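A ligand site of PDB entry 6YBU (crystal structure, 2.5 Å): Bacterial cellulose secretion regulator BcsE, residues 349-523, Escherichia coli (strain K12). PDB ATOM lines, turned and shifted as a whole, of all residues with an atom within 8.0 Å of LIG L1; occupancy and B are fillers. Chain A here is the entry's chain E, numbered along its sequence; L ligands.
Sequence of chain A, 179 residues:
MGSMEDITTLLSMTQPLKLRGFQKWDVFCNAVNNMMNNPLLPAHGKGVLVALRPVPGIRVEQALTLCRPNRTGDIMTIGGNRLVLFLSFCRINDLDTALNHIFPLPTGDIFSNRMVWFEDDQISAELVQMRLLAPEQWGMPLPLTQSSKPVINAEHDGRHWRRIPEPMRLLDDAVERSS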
ATOM      1  N   LEU A  17       5.307 -20.056  -1.318  1.00  0.00           N
ATOM      2  CA  LEU A  17       6.113 -20.716  -2.338  1.00  0.00           C
ATOM      3  C   LEU A  17       5.661 -20.419  -3.756  1.00  0.00           C
ATOM      4  O   LEU A  17       6.305 -20.885  -4.703  1.00  0.00           O
ATOM      5  CB  LEU A  17       6.118 -22.232  -2.089  1.00  0.00           C
ATOM      6  CG  LEU A  17       6.780 -22.674  -0.791  1.00  0.00           C
ATOM      7  CD1 LEU A  17       6.614 -24.167  -0.566  1.00  0.00           C
ATOM      8  CD2 LEU A  17       8.256 -22.288  -0.793  1.00  0.00           C
ATOM      9  N   LEU A  19       5.204 -17.152  -4.801  1.00  0.00           N
ATOM     10  CA  LEU A  19       5.775 -15.862  -5.175  1.00  0.00           C
ATOM     11  C   LEU A  19       7.055 -16.056  -5.983  1.00  0.00           C
ATOM     12  O   LEU A  19       7.731 -17.079  -5.896  1.00  0.00           O
ATOM     13  CB  LEU A  19       6.071 -15.033  -3.923  1.00  0.00           C
ATOM     14  CG  LEU A  19       4.881 -14.579  -3.070  1.00  0.00           C
ATOM     15  CD1 LEU A  19       5.353 -14.107  -1.706  1.00  0.00           C
ATOM     16  CD2 LEU A  19       4.109 -13.481  -3.783  1.00  0.00           C
ATOM     17  N   ARG A  20       7.380 -15.033  -6.767  1.00  0.00           N
ATOM     18  CA  ARG A  20       8.686 -14.954  -7.418  1.00  0.00           C
ATOM     19  C   ARG A  20       8.987 -13.491  -7.704  1.00  0.00           C
ATOM     20  O   ARG A  20       8.087 -12.661  -7.818  1.00  0.00           O
ATOM     21  CB  ARG A  20       8.753 -15.776  -8.713  1.00  0.00           C
ATOM     22  CG  ARG A  20      10.183 -16.174  -9.082  1.00  0.00           C
ATOM     23  CD  ARG A  20      10.480 -15.993 -10.567  1.00  0.00           C
ATOM     24  NE  ARG A  20       9.850 -17.027 -11.384  1.00  0.00           N
ATOM     25  CZ  ARG A  20       8.880 -16.791 -12.261  1.00  0.00           C
ATOM     26  NH1 ARG A  20       8.420 -15.561 -12.431  1.00  0.00           N
ATOM     27  NH2 ARG A  20       8.367 -17.798 -12.970  1.00  0.00           N
ATOM     28  N   ARG A  68      17.558 -11.817 -11.612  1.00  0.00           N
ATOM     29  CA  ARG A  68      16.522 -12.372 -12.480  1.00  0.00           C
ATOM     30  C   ARG A  68      16.316 -13.853 -12.159  1.00  0.00           C
ATOM     31  O   ARG A  68      16.763 -14.735 -12.893  1.00  0.00           O
ATOM     32  CB  ARG A  68      16.887 -12.192 -13.948  1.00  0.00           C
ATOM     33  CG  ARG A  68      16.999 -10.733 -14.355  1.00  0.00           C
ATOM     34  CD  ARG A  68      17.866 -10.552 -15.598  1.00  0.00           C
ATOM     35  NE  ARG A  68      18.159  -9.147 -15.839  1.00  0.00           N
ATOM     36  CZ  ARG A  68      19.032  -8.704 -16.739  1.00  0.00           C
ATOM     37  NH1 ARG A  68      19.229  -7.396 -16.885  1.00  0.00           N
ATOM     38  NH2 ARG A  68      19.710  -9.554 -17.491  1.00  0.00           N
ATOM     39  N   PRO A  69      15.616 -14.153 -11.067  1.00  0.00           N
ATOM     40  CA  PRO A  69      15.335 -15.551 -10.726  1.00  0.00           C
ATOM     41  C   PRO A  69      14.239 -16.128 -11.609  1.00  0.00           C
ATOM     42  O   PRO A  69      13.354 -15.418 -12.097  1.00  0.00           O
ATOM     43  CB  PRO A  69      14.877 -15.467  -9.267  1.00  0.00           C
ATOM     44  CG  PRO A  69      14.189 -14.160  -9.220  1.00  0.00           C
ATOM     45  CD  PRO A  69      15.005 -13.230 -10.088  1.00  0.00           C
ATOM     46  N   ASN A  70      14.302 -17.445 -11.784  1.00  0.00           N
ATOM     47  CA  ASN A  70      13.322 -18.172 -12.589  1.00  0.00           C
ATOM     48  C   ASN A  70      12.559 -19.222 -11.801  1.00  0.00           C
ATOM     49  O   ASN A  70      11.395 -19.468 -12.100  1.00  0.00           O
ATOM     50  CB  ASN A  70      14.022 -18.841 -13.780  1.00  0.00           C
ATOM     51  CG  ASN A  70      15.053 -17.943 -14.430  1.00  0.00           C
ATOM     52  OD1 ASN A  70      14.715 -17.009 -15.153  1.00  0.00           O
ATOM     53  ND2 ASN A  70      16.323 -18.244 -14.186  1.00  0.00           N
ATOM     54  N   ARG A  71      13.191 -19.842 -10.809  1.00  0.00           N
ATOM     55  CA  ARG A  71      12.534 -20.841  -9.974  1.00  0.00           C
ATOM     56  C   ARG A  71      11.427 -20.186  -9.149  1.00  0.00           C
ATOM     57  O   ARG A  71      11.684 -19.222  -8.408  1.00  0.00           O
ATOM     58  CB  ARG A  71      13.552 -21.509  -9.068  1.00  0.00           C
ATOM     59  CG  ARG A  71      13.054 -22.644  -8.191  1.00  0.00           C
ATOM     60  CD  ARG A  71      14.049 -23.785  -8.252  1.00  0.00           C
ATOM     61  NE  ARG A  71      14.223 -24.530  -7.010  1.00  0.00           N
ATOM     62  CZ  ARG A  71      14.985 -25.612  -6.900  1.00  0.00           C
ATOM     63  NH1 ARG A  71      15.094 -26.247  -5.746  1.00  0.00           N
ATOM     64  NH2 ARG A  71      15.639 -26.056  -7.967  1.00  0.00           N
ATOM     65  N   THR A  72      10.201 -20.677  -9.286  1.00  0.00           N
ATOM     66  CA  THR A  72       9.103 -20.180  -8.461  1.00  0.00           C
ATOM     67  C   THR A  72       9.404 -20.452  -6.995  1.00  0.00           C
ATOM     68  O   THR A  72       9.820 -21.563  -6.632  1.00  0.00           O
ATOM     69  CB  THR A  72       7.778 -20.824  -8.872  1.00  0.00           C
ATOM     70  OG1 THR A  72       7.493 -20.502 -10.236  1.00  0.00           O
ATOM     71  CG2 THR A  72       6.649 -20.313  -7.991  1.00  0.00           C
ATOM     72  N   GLY A  73       9.205 -19.442  -6.162  1.00  0.00           N
ATOM     73  CA  GLY A  73       9.611 -19.498  -4.770  1.00  0.00           C
ATOM     74  C   GLY A  73      10.890 -18.744  -4.471  1.00  0.00           C
ATOM     75  O   GLY A  73      11.189 -18.530  -3.290  1.00  0.00           O
ATOM     76  N   ASP A  74      11.635 -18.339  -5.497  1.00  0.00           N
ATOM     77  CA  ASP A  74      12.792 -17.474  -5.312  1.00  0.00           C
ATOM     78  C   ASP A  74      12.328 -16.027  -5.314  1.00  0.00           C
ATOM     79  O   ASP A  74      11.684 -15.572  -6.271  1.00  0.00           O
ATOM     80  CB  ASP A  74      13.817 -17.699  -6.426  1.00  0.00           C
ATOM     81  CG  ASP A  74      14.502 -19.058  -6.312  1.00  0.00           C
ATOM     82  OD1 ASP A  74      14.209 -19.796  -5.362  1.00  0.00           O
ATOM     83  OD2 ASP A  74      15.341 -19.374  -7.195  1.00  0.00           O
ATOM     84  N   SER A  88      14.375 -20.828  -2.575  1.00  0.00           N
ATOM     85  CA  SER A  88      13.539 -21.887  -2.014  1.00  0.00           C
ATOM     86  C   SER A  88      14.148 -23.260  -2.267  1.00  0.00           C
ATOM     87  O   SER A  88      14.457 -23.613  -3.420  1.00  0.00           O
ATOM     88  CB  SER A  88      12.132 -21.817  -2.588  1.00  0.00           C
ATOM     89  OG  SER A  88      12.143 -21.987  -3.999  1.00  0.00           O
ATOM     90  N   PHE A  89      14.338 -24.025  -1.189  1.00  0.00           N
ATOM     91  CA  PHE A  89      14.798 -25.419  -1.237  1.00  0.00           C
ATOM     92  C   PHE A  89      16.160 -25.565  -1.900  1.00  0.00           C
ATOM     93  O   PHE A  89      16.513 -26.654  -2.366  1.00  0.00           O
ATOM     94  CB  PHE A  89      13.749 -26.304  -1.924  1.00  0.00           C
ATOM     95  CG  PHE A  89      12.387 -26.153  -1.343  1.00  0.00           C
ATOM     96  CD1 PHE A  89      12.108 -26.620  -0.077  1.00  0.00           C
ATOM     97  CD2 PHE A  89      11.382 -25.526  -2.061  1.00  0.00           C
ATOM     98  CE1 PHE A  89      10.852 -26.469   0.475  1.00  0.00           C
ATOM     99  CE2 PHE A  89      10.121 -25.374  -1.518  1.00  0.00           C
ATOM    100  CZ  PHE A  89       9.854 -25.835  -0.247  1.00  0.00           C
ATOM    101  N   CYS A  90      16.929 -24.482  -1.960  1.00  0.00           N
ATOM    102  CA  CYS A  90      18.309 -24.556  -2.438  1.00  0.00           C
ATOM    103  C   CYS A  90      19.205 -25.043  -1.309  1.00  0.00           C
ATOM    104  O   CYS A  90      19.211 -24.478  -0.216  1.00  0.00           O
ATOM    105  CB  CYS A  90      18.767 -23.179  -2.923  1.00  0.00           C
ATOM    106  SG  CYS A  90      20.522 -23.083  -3.327  1.00  0.00           S
ATOM    107  N   THR A  97      25.749 -22.135  -7.444  1.00  0.00           N
ATOM    108  CA  THR A  97      25.058 -22.585  -8.651  1.00  0.00           C
ATOM    109  C   THR A  97      23.778 -21.801  -8.869  1.00  0.00           C
ATOM    110  O   THR A  97      23.540 -21.259  -9.954  1.00  0.00           O
ATOM    111  CB  THR A  97      24.773 -24.088  -8.566  1.00  0.00           C
ATOM    112  OG1 THR A  97      25.987 -24.825  -8.667  1.00  0.00           O
ATOM    113  CG2 THR A  97      23.836 -24.507  -9.691  1.00  0.00           C
ATOM    114  N   ALA A  98      22.930 -21.729  -7.832  1.00  0.00           N
ATOM    115  CA  ALA A  98      21.679 -20.983  -7.943  1.00  0.00           C
ATOM    116  C   ALA A  98      21.940 -19.509  -8.227  1.00  0.00           C
ATOM    117  O   ALA A  98      21.261 -18.902  -9.063  1.00  0.00           O
ATOM    118  CB  ALA A  98      20.852 -21.141  -6.663  1.00  0.00           C
ATOM    119  N   HIS A 101      22.777 -18.827 -11.789  1.00  0.00           N
ATOM    120  CA  HIS A 101      21.606 -18.880 -12.660  1.00  0.00           C
ATOM    121  C   HIS A 101      20.773 -17.612 -12.589  1.00  0.00           C
ATOM    122  O   HIS A 101      20.040 -17.306 -13.544  1.00  0.00           O
ATOM    123  CB  HIS A 101      20.732 -20.078 -12.315  1.00  0.00           C
ATOM    124  CG  HIS A 101      21.345 -21.404 -12.648  1.00  0.00           C
ATOM    125  ND1 HIS A 101      20.971 -22.570 -12.014  1.00  0.00           N
ATOM    126  CD2 HIS A 101      22.299 -21.749 -13.544  1.00  0.00           C
ATOM    127  CE1 HIS A 101      21.669 -23.580 -12.503  1.00  0.00           C
ATOM    128  NE2 HIS A 101      22.484 -23.109 -13.434  1.00  0.00           N
HETATM  129  P1  LIG L   1      11.906 -25.505 -17.047  1.00  0.00           P
HETATM  130  O1  LIG L   1      13.188 -26.308 -16.867  1.00  0.00           O
HETATM  131  O2  LIG L   1      11.404 -25.412 -18.435  1.00  0.00           O
HETATM  132  O3  LIG L   1      10.826 -26.172 -16.048  1.00  0.00           O
HETATM  133  C1  LIG L   1       9.445 -25.785 -15.909  1.00  0.00           C
HETATM  134  C2  LIG L   1       8.938 -26.294 -14.581  1.00  0.00           C
HETATM  135  O4  LIG L   1       8.977 -27.734 -14.568  1.00  0.00           O
HETATM  136  C3  LIG L   1       9.788 -25.885 -13.381  1.00  0.00           C
HETATM  137  O5  LIG L   1       9.337 -24.620 -12.872  1.00  0.00           O
HETATM  138  C4  LIG L   1       9.465 -26.980 -12.371  1.00  0.00           C
HETATM  139  O6  LIG L   1       8.211 -26.748 -11.740  1.00  0.00           O
HETATM  140  C5  LIG L   1       9.377 -28.209 -13.290  1.00  0.00           C
HETATM  141  N1  LIG L   1      10.654 -28.913 -13.437  1.00  0.00           N
HETATM  142  C6  LIG L   1      11.516 -28.850 -14.502  1.00  0.00           C
HETATM  143  N2  LIG L   1      12.583 -29.604 -14.352  1.00  0.00           N
HETATM  144  C7  LIG L   1      12.411 -30.200 -13.106  1.00  0.00           C
HETATM  145  C8  LIG L   1      13.233 -31.124 -12.392  1.00  0.00           C
HETATM  146  O7  LIG L   1      14.312 -31.599 -12.746  1.00  0.00           O
HETATM  147  N3  LIG L   1      12.684 -31.466 -11.172  1.00  0.00           N
HETATM  148  C9  LIG L   1      11.496 -30.997 -10.683  1.00  0.00           C
HETATM  149  N4  LIG L   1      11.119 -31.444  -9.485  1.00  0.00           N
HETATM  150  N5  LIG L   1      10.722 -30.137 -11.340  1.00  0.00           N
HETATM  151  C10 LIG L   1      11.229 -29.786 -12.534  1.00  0.00           C
HETATM  152  P2  LIG L   1      10.075 -23.544 -11.963  1.00  0.00           P
HETATM  153  O8  LIG L   1      10.617 -24.298 -10.756  1.00  0.00           O
HETATM  154  O9  LIG L   1       9.201 -22.403 -11.623  1.00  0.00           O
HETATM  155  O10 LIG L   1      11.360 -23.101 -12.854  1.00  0.00           O
HETATM  156  C11 LIG L   1      11.332 -22.157 -13.939  1.00  0.00           C
HETATM  157  C12 LIG L   1      12.578 -22.304 -14.779  1.00  0.00           C
HETATM  158  O11 LIG L   1      13.745 -21.924 -14.009  1.00  0.00           O
HETATM  159  C13 LIG L   1      12.895 -23.718 -15.224  1.00  0.00           C
HETATM  160  O12 LIG L   1      12.172 -24.073 -16.423  1.00  0.00           O
HETATM  161  C14 LIG L   1      14.395 -23.651 -15.500  1.00  0.00           C
HETATM  162  O13 LIG L   1      14.653 -23.006 -16.745  1.00  0.00           O
HETATM  163  C15 LIG L   1      14.843 -22.759 -14.332  1.00  0.00           C
HETATM  164  N6  LIG L   1      15.192 -23.537 -13.140  1.00  0.00           N
HETATM  165  C16 LIG L   1      14.466 -23.632 -11.985  1.00  0.00           C
HETATM  166  N7  LIG L   1      15.028 -24.404 -11.085  1.00  0.00           N
HETATM  167  C17 LIG L   1      16.191 -24.843 -11.685  1.00  0.00           C
HETATM  168  C18 LIG L   1      17.214 -25.706 -11.203  1.00  0.00           C
HETATM  169  O14 LIG L   1      17.283 -26.250 -10.097  1.00  0.00           O
HETATM  170  N8  LIG L   1      18.231 -25.892 -12.131  1.00  0.00           N
HETATM  171  C19 LIG L   1      18.255 -25.326 -13.373  1.00  0.00           C
HETATM  172  N9  LIG L   1      19.311 -25.610 -14.148  1.00  0.00           N
HETATM  173  N10 LIG L   1      17.308 -24.513 -13.836  1.00  0.00           N
HETATM  174  C20 LIG L   1      16.312 -24.320 -12.942  1.00  0.00           C
HETATM  175  P1  LG2 L   2      21.897 -27.755 -11.070  1.00  0.00           P
HETATM  176  O1  LG2 L   2      21.205 -26.831 -12.074  1.00  0.00           O
HETATM  177  O2  LG2 L   2      23.353 -27.904 -11.239  1.00  0.00           O
HETATM  178  O3  LG2 L   2      21.506 -27.244  -9.603  1.00  0.00           O
HETATM  179  C1  LG2 L   2      21.948 -27.876  -8.380  1.00  0.00           C
HETATM  180  C2  LG2 L   2      21.097 -27.420  -7.228  1.00  0.00           C
HETATM  181  O4  LG2 L   2      21.212 -25.997  -7.054  1.00  0.00           O
HETATM  182  C3  LG2 L   2      19.590 -27.636  -7.399  1.00  0.00           C
HETATM  183  O5  LG2 L   2      19.244 -28.964  -6.952  1.00  0.00           O
HETATM  184  C4  LG2 L   2      19.011 -26.616  -6.429  1.00  0.00           C
HETATM  185  O6  LG2 L   2      19.093 -27.090  -5.088  1.00  0.00           O
HETATM  186  C5  LG2 L   2      19.978 -25.441  -6.633  1.00  0.00           C
HETATM  187  N1  LG2 L   2      19.529 -24.480  -7.650  1.00  0.00           N
HETATM  188  C6  LG2 L   2      20.040 -24.332  -8.916  1.00  0.00           C
HETATM  189  N2  LG2 L   2      19.482 -23.347  -9.583  1.00  0.00           N
HETATM  190  C7  LG2 L   2      18.539 -22.830  -8.708  1.00  0.00           C
HETATM  191  C8  LG2 L   2      17.630 -21.735  -8.845  1.00  0.00           C
HETATM  192  O7  LG2 L   2      17.501 -20.995  -9.822  1.00  0.00           O
HETATM  193  N3  LG2 L   2      16.861 -21.547  -7.714  1.00  0.00           N
HETATM  194  C9  LG2 L   2      16.949 -22.301  -6.573  1.00  0.00           C
HETATM  195  N4  LG2 L   2      16.119 -21.979  -5.566  1.00  0.00           N
HETATM  196  N5  LG2 L   2      17.789 -23.320  -6.421  1.00  0.00           N
HETATM  197  C10 LG2 L   2      18.554 -23.517  -7.516  1.00  0.00           C
HETATM  198  P2  LG2 L   2      18.036 -29.910  -7.351  1.00  0.00           P
HETATM  199  O8  LG2 L   2      16.762 -29.069  -7.249  1.00  0.00           O
HETATM  200  O9  LG2 L   2      18.004 -31.152  -6.545  1.00  0.00           O
HETATM  201  O10 LG2 L   2      18.267 -30.210  -8.921  1.00  0.00           O
HETATM  202  C11 LG2 L   2      19.225 -31.140  -9.452  1.00  0.00           C
HETATM  203  C12 LG2 L   2      19.407 -30.872 -10.929  1.00  0.00           C
HETATM  204  O11 LG2 L   2      18.166 -31.115 -11.627  1.00  0.00           O
HETATM  205  C13 LG2 L   2      19.740 -29.435 -11.296  1.00  0.00           C
HETATM  206  O12 LG2 L   2      21.156 -29.165 -11.170  1.00  0.00           O
HETATM  207  C14 LG2 L   2      19.310 -29.372 -12.755  1.00  0.00           C
HETATM  208  O13 LG2 L   2      20.274 -30.007 -13.585  1.00  0.00           O
HETATM  209  C15 LG2 L   2      18.030 -30.205 -12.697  1.00  0.00           C
HETATM  210  N6  LG2 L   2      16.820 -29.392 -12.461  1.00  0.00           N
HETATM  211  C16 LG2 L   2      16.059 -29.369 -11.319  1.00  0.00           C
HETATM  212  N7  LG2 L   2      15.009 -28.577 -11.416  1.00  0.00           N
HETATM  213  C17 LG2 L   2      15.097 -28.050 -12.701  1.00  0.00           C
HETATM  214  C18 LG2 L   2      14.249 -27.138 -13.401  1.00  0.00           C
HETATM  215  O14 LG2 L   2      13.209 -26.621 -12.972  1.00  0.00           O
HETATM  216  N8  LG2 L   2      14.708 -26.864 -14.668  1.00  0.00           N
HETATM  217  C19 LG2 L   2      15.838 -27.402 -15.235  1.00  0.00           C
HETATM  218  N9  LG2 L   2      16.136 -27.017 -16.475  1.00  0.00           N
HETATM  219  N10 LG2 L   2      16.635 -28.263 -14.593  1.00  0.00           N
HETATM  220  C20 LG2 L   2      16.206 -28.545 -13.345  1.00  0.00           C
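Merely in contact with LIG L1: Asn 70 and His 101.
Four residues have an atom within 4 Å of LIG L1: Asn 70, Arg 71, Thr 72 and His 101.
The nearest printed residue that does not touch LIG L1 is Arg 20 (4.9 Å).
An oxygen (O1) of LIG L1 lies within hydrogen-bond range of a nitrogen (N8) of LG2 L2 (2.7 Å).
O of Asn 70 sits at hydrogen-bond distance from NE of Arg 20 (3.0 Å).
The guanidinium group (NH2) of Arg 71 lies within salt-bridge range of an oxygen (O8) of LG2 L2 (3.3 Å).
O9 of LIG L1 sits at hydrogen-bond distance from N of Thr 72 (3.1 Å).
The backbone carbonyl oxygen (O) of Ser 88 sits at hydrogen-bond distance from a nitrogen (N4) of LG2 L2, 3.2 Å away.
The side-chain carboxylate (OD2) of Asp 74 lies within hydrogen-bond range of a nitrogen (N3) of LG2 L2.
The side-chain hydroxyl (OG1) of Thr 72 lies within hydrogen-bond range of an oxygen (O9) of LIG L1, at 2.9 Å.
NH2 of Arg 71 lies within hydrogen-bond range of O14 of LIG L1 (2.7 Å).
ND1 of His 101 is in hydrogen-bond range of N2 of LG2 L2, 3.0 Å away.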
